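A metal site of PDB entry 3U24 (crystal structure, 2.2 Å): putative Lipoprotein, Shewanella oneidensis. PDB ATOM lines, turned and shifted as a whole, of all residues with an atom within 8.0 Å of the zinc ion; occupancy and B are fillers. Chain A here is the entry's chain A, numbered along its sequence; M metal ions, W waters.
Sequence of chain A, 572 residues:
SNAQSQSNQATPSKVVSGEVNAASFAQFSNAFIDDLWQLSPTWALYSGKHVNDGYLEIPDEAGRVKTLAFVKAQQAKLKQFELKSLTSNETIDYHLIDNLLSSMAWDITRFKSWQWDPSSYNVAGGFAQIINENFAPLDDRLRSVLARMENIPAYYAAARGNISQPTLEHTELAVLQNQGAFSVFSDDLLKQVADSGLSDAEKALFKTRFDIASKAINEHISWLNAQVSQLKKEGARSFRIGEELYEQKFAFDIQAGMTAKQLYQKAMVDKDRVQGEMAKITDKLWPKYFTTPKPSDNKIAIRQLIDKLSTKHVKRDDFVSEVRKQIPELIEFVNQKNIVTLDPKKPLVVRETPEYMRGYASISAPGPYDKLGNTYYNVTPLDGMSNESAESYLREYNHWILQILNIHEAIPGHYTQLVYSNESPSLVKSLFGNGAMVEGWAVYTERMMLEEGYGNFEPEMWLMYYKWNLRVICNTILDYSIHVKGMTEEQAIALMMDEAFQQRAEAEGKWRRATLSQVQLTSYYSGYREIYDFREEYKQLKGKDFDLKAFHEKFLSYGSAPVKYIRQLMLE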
ATOM      1  N   ALA A 361     -20.503  16.893 -25.523  1.00  0.00           N
ATOM      2  CA  ALA A 361     -21.773  17.115 -26.223  1.00  0.00           C
ATOM      3  C   ALA A 361     -21.700  18.349 -27.116  1.00  0.00           C
ATOM      4  O   ALA A 361     -21.419  19.450 -26.648  1.00  0.00           O
ATOM      5  CB  ALA A 361     -22.908  17.222 -25.238  1.00  0.00           C
ATOM      6  N   SER A 362     -21.916  18.166 -28.421  1.00  0.00           N
ATOM      7  CA  SER A 362     -21.915  19.298 -29.391  1.00  0.00           C
ATOM      8  C   SER A 362     -22.697  19.025 -30.676  1.00  0.00           C
ATOM      9  O   SER A 362     -22.980  17.888 -31.025  1.00  0.00           O
ATOM     10  CB  SER A 362     -20.479  19.704 -29.735  1.00  0.00           C
ATOM     11  OG  SER A 362     -19.860  18.756 -30.579  1.00  0.00           O
ATOM     12  N   LEU A 405     -26.246  22.938 -20.107  1.00  0.00           N
ATOM     13  CA  LEU A 405     -25.528  22.465 -21.311  1.00  0.00           C
ATOM     14  C   LEU A 405     -26.458  22.299 -22.526  1.00  0.00           C
ATOM     15  O   LEU A 405     -26.085  22.629 -23.667  1.00  0.00           O
ATOM     16  CB  LEU A 405     -24.811  21.124 -21.057  1.00  0.00           C
ATOM     17  CG  LEU A 405     -24.080  20.454 -22.246  1.00  0.00           C
ATOM     18  CD1 LEU A 405     -22.830  21.244 -22.637  1.00  0.00           C
ATOM     19  CD2 LEU A 405     -23.719  18.991 -21.977  1.00  0.00           C
ATOM     20  N   HIS A 408     -27.379  25.671 -23.923  1.00  0.00           N
ATOM     21  CA  HIS A 408     -26.231  26.225 -24.626  1.00  0.00           C
ATOM     22  C   HIS A 408     -26.091  25.566 -25.968  1.00  0.00           C
ATOM     23  O   HIS A 408     -25.896  26.233 -26.985  1.00  0.00           O
ATOM     24  CB  HIS A 408     -24.942  26.036 -23.809  1.00  0.00           C
ATOM     25  CG  HIS A 408     -23.656  26.510 -24.491  1.00  0.00           C
ATOM     26  ND1 HIS A 408     -22.987  27.602 -24.087  1.00  0.00           N
ATOM     27  CD2 HIS A 408     -22.938  26.002 -25.585  1.00  0.00           C
ATOM     28  CE1 HIS A 408     -21.875  27.797 -24.901  1.00  0.00           C
ATOM     29  NE2 HIS A 408     -21.841  26.833 -25.798  1.00  0.00           N
ATOM     30  N   GLU A 409     -26.152  24.250 -25.991  1.00  0.00           N
ATOM     31  CA  GLU A 409     -25.830  23.499 -27.204  1.00  0.00           C
ATOM     32  C   GLU A 409     -26.985  23.342 -28.173  1.00  0.00           C
ATOM     33  O   GLU A 409     -26.789  23.318 -29.369  1.00  0.00           O
ATOM     34  CB  GLU A 409     -25.323  22.087 -26.837  1.00  0.00           C
ATOM     35  CG  GLU A 409     -23.969  22.096 -26.164  1.00  0.00           C
ATOM     36  CD  GLU A 409     -22.883  22.572 -27.083  1.00  0.00           C
ATOM     37  OE1 GLU A 409     -23.094  22.445 -28.313  1.00  0.00           O
ATOM     38  OE2 GLU A 409     -21.839  23.054 -26.608  1.00  0.00           O
ATOM     39  N   GLY A 413     -29.871  27.717 -27.851  1.00  0.00           N
ATOM     40  CA  GLY A 413     -28.473  28.036 -28.154  1.00  0.00           C
ATOM     41  C   GLY A 413     -27.962  27.653 -29.553  1.00  0.00           C
ATOM     42  O   GLY A 413     -28.567  28.037 -30.608  1.00  0.00           O
ATOM     43  N   HIS A 414     -26.872  26.884 -29.597  1.00  0.00           N
ATOM     44  CA  HIS A 414     -26.202  26.669 -30.901  1.00  0.00           C
ATOM     45  C   HIS A 414     -27.070  26.146 -31.987  1.00  0.00           C
ATOM     46  O   HIS A 414     -26.978  26.649 -33.089  1.00  0.00           O
ATOM     47  CB  HIS A 414     -24.997  25.748 -30.789  1.00  0.00           C
ATOM     48  CG  HIS A 414     -23.840  26.385 -30.115  1.00  0.00           C
ATOM     49  ND1 HIS A 414     -23.465  27.654 -30.375  1.00  0.00           N
ATOM     50  CD2 HIS A 414     -22.964  25.898 -29.179  1.00  0.00           C
ATOM     51  CE1 HIS A 414     -22.412  27.950 -29.611  1.00  0.00           C
ATOM     52  NE2 HIS A 414     -22.070  26.847 -28.935  1.00  0.00           N
ATOM     53  N   GLY A 435     -16.712  33.688 -34.363  1.00  0.00           N
ATOM     54  CA  GLY A 435     -16.827  32.750 -33.262  1.00  0.00           C
ATOM     55  C   GLY A 435     -17.367  33.398 -32.000  1.00  0.00           C
ATOM     56  O   GLY A 435     -18.133  32.789 -31.243  1.00  0.00           O
ATOM     57  N   VAL A 438     -21.186  33.484 -32.154  1.00  0.00           N
ATOM     58  CA  VAL A 438     -21.765  32.148 -32.094  1.00  0.00           C
ATOM     59  C   VAL A 438     -21.731  31.643 -30.656  1.00  0.00           C
ATOM     60  O   VAL A 438     -22.758  31.225 -30.079  1.00  0.00           O
ATOM     61  CB  VAL A 438     -21.041  31.188 -33.073  1.00  0.00           C
ATOM     62  CG1 VAL A 438     -21.337  29.700 -32.788  1.00  0.00           C
ATOM     63  CG2 VAL A 438     -21.321  31.601 -34.538  1.00  0.00           C
ATOM     64  N   GLU A 439     -20.587  31.780 -30.035  1.00  0.00           N
ATOM     65  CA  GLU A 439     -20.473  31.377 -28.639  1.00  0.00           C
ATOM     66  C   GLU A 439     -21.201  32.342 -27.691  1.00  0.00           C
ATOM     67  O   GLU A 439     -21.865  31.885 -26.748  1.00  0.00           O
ATOM     68  CB  GLU A 439     -19.008  31.240 -28.207  1.00  0.00           C
ATOM     69  CG  GLU A 439     -18.405  29.956 -28.711  1.00  0.00           C
ATOM     70  CD  GLU A 439     -19.133  28.713 -28.197  1.00  0.00           C
ATOM     71  OE1 GLU A 439     -19.779  28.752 -27.099  1.00  0.00           O
ATOM     72  OE2 GLU A 439     -19.043  27.675 -28.893  1.00  0.00           O
ATOM     73  N   GLY A 440     -21.046  33.655 -27.917  1.00  0.00           N
ATOM     74  CA  GLY A 440     -21.740  34.652 -27.084  1.00  0.00           C
ATOM     75  C   GLY A 440     -23.240  34.435 -27.039  1.00  0.00           C
ATOM     76  O   GLY A 440     -23.854  34.543 -25.994  1.00  0.00           O
ATOM     77  N   TRP A 441     -23.829  34.111 -28.200  1.00  0.00           N
ATOM     78  CA  TRP A 441     -25.233  33.783 -28.255  1.00  0.00           C
ATOM     79  C   TRP A 441     -25.559  32.612 -27.342  1.00  0.00           C
ATOM     80  O   TRP A 441     -26.534  32.657 -26.566  1.00  0.00           O
ATOM     81  CB  TRP A 441     -25.688  33.484 -29.687  1.00  0.00           C
ATOM     82  CG  TRP A 441     -27.063  32.927 -29.715  1.00  0.00           C
ATOM     83  CD1 TRP A 441     -27.430  31.595 -29.781  1.00  0.00           C
ATOM     84  CD2 TRP A 441     -28.330  33.662 -29.520  1.00  0.00           C
ATOM     85  NE1 TRP A 441     -28.792  31.464 -29.698  1.00  0.00           N
ATOM     86  CE2 TRP A 441     -29.386  32.661 -29.531  1.00  0.00           C
ATOM     87  CE3 TRP A 441     -28.664  34.993 -29.363  1.00  0.00           C
ATOM     88  CZ2 TRP A 441     -30.711  33.007 -29.392  1.00  0.00           C
ATOM     89  CZ3 TRP A 441     -30.005  35.320 -29.187  1.00  0.00           C
ATOM     90  CH2 TRP A 441     -31.008  34.352 -29.218  1.00  0.00           C
ATOM     91  N   ALA A 442     -24.784  31.530 -27.433  1.00  0.00           N
ATOM     92  CA  ALA A 442     -25.083  30.351 -26.649  1.00  0.00           C
ATOM     93  C   ALA A 442     -24.990  30.660 -25.168  1.00  0.00           C
ATOM     94  O   ALA A 442     -25.869  30.252 -24.433  1.00  0.00           O
ATOM     95  CB  ALA A 442     -24.174  29.183 -27.014  1.00  0.00           C
ATOM     96  N   VAL A 443     -23.958  31.398 -24.745  1.00  0.00           N
ATOM     97  CA  VAL A 443     -23.826  31.839 -23.313  1.00  0.00           C
ATOM     98  C   VAL A 443     -24.966  32.750 -22.866  1.00  0.00           C
ATOM     99  O   VAL A 443     -25.552  32.584 -21.786  1.00  0.00           O
ATOM    100  CB  VAL A 443     -22.449  32.491 -23.067  1.00  0.00           C
ATOM    101  CG1 VAL A 443     -22.249  32.964 -21.612  1.00  0.00           C
ATOM    102  CG2 VAL A 443     -21.348  31.508 -23.504  1.00  0.00           C
ATOM    103  N   GLU A 446     -28.285  30.952 -21.859  1.00  0.00           N
ATOM    104  CA  GLU A 446     -28.329  30.387 -20.538  1.00  0.00           C
ATOM    105  C   GLU A 446     -28.918  31.424 -19.533  1.00  0.00           C
ATOM    106  O   GLU A 446     -29.854  31.131 -18.783  1.00  0.00           O
ATOM    107  CB  GLU A 446     -26.933  29.958 -20.089  1.00  0.00           C
ATOM    108  CG  GLU A 446     -26.167  29.117 -21.106  1.00  0.00           C
ATOM    109  CD  GLU A 446     -24.667  29.049 -20.828  1.00  0.00           C
ATOM    110  OE1 GLU A 446     -24.207  29.668 -19.849  1.00  0.00           O
ATOM    111  OE2 GLU A 446     -23.940  28.363 -21.602  1.00  0.00           O
ATOM    112  N   ARG A 471     -16.714  30.280 -15.290  1.00  0.00           N
ATOM    113  CA  ARG A 471     -15.784  29.691 -16.269  1.00  0.00           C
ATOM    114  C   ARG A 471     -15.479  30.709 -17.394  1.00  0.00           C
ATOM    115  O   ARG A 471     -14.331  30.916 -17.816  1.00  0.00           O
ATOM    116  CB  ARG A 471     -16.446  28.455 -16.890  1.00  0.00           C
ATOM    117  CG  ARG A 471     -15.573  27.260 -17.253  1.00  0.00           C
ATOM    118  CD  ARG A 471     -16.455  26.001 -17.467  1.00  0.00           C
ATOM    119  NE  ARG A 471     -16.913  25.822 -18.864  1.00  0.00           N
ATOM    120  CZ  ARG A 471     -17.995  26.365 -19.458  1.00  0.00           C
ATOM    121  NH1 ARG A 471     -18.245  26.096 -20.741  1.00  0.00           N
ATOM    122  NH2 ARG A 471     -18.837  27.187 -18.810  1.00  0.00           N
ATOM    123  N   TYR A 524     -15.892  33.714 -25.585  1.00  0.00           N
ATOM    124  CA  TYR A 524     -17.162  33.349 -24.947  1.00  0.00           C
ATOM    125  C   TYR A 524     -17.758  34.535 -24.221  1.00  0.00           C
ATOM    126  O   TYR A 524     -18.936  34.887 -24.433  1.00  0.00           O
ATOM    127  CB  TYR A 524     -16.984  32.188 -23.987  1.00  0.00           C
ATOM    128  CG  TYR A 524     -16.209  31.059 -24.598  1.00  0.00           C
ATOM    129  CD1 TYR A 524     -14.803  31.051 -24.536  1.00  0.00           C
ATOM    130  CD2 TYR A 524     -16.848  30.003 -25.228  1.00  0.00           C
ATOM    131  CE1 TYR A 524     -14.072  30.050 -25.109  1.00  0.00           C
ATOM    132  CE2 TYR A 524     -16.124  28.984 -25.813  1.00  0.00           C
ATOM    133  CZ  TYR A 524     -14.751  29.002 -25.746  1.00  0.00           C
ATOM    134  OH  TYR A 524     -13.987  28.028 -26.302  1.00  0.00           O
HETATM  135 ZN    ZN M   1     -20.695  26.816 -27.295  1.00  0.00          ZN
HETATM  136  O   HOH W   1     -19.960  24.819 -27.216  1.00  0.00           O
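A ring nitrogen (ND1) of His 408 sits at hydrogen-bond distance from the side-chain carboxylate (OE2) of Glu 446, 2.8 Å away.
Residues that only touch the zinc ion: Glu 409. Within 4 Å of the zinc ion: His 408, Glu 409, His 414 and Glu 439.
The zinc ion is bound by NE2 of His 408 (1.9 Å), water W1 (2.1 Å), NE2 of His 414 (2.1 Å), OE1 of Glu 439 (2.2 Å) and OE2 of Glu 439 (2.5 Å).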
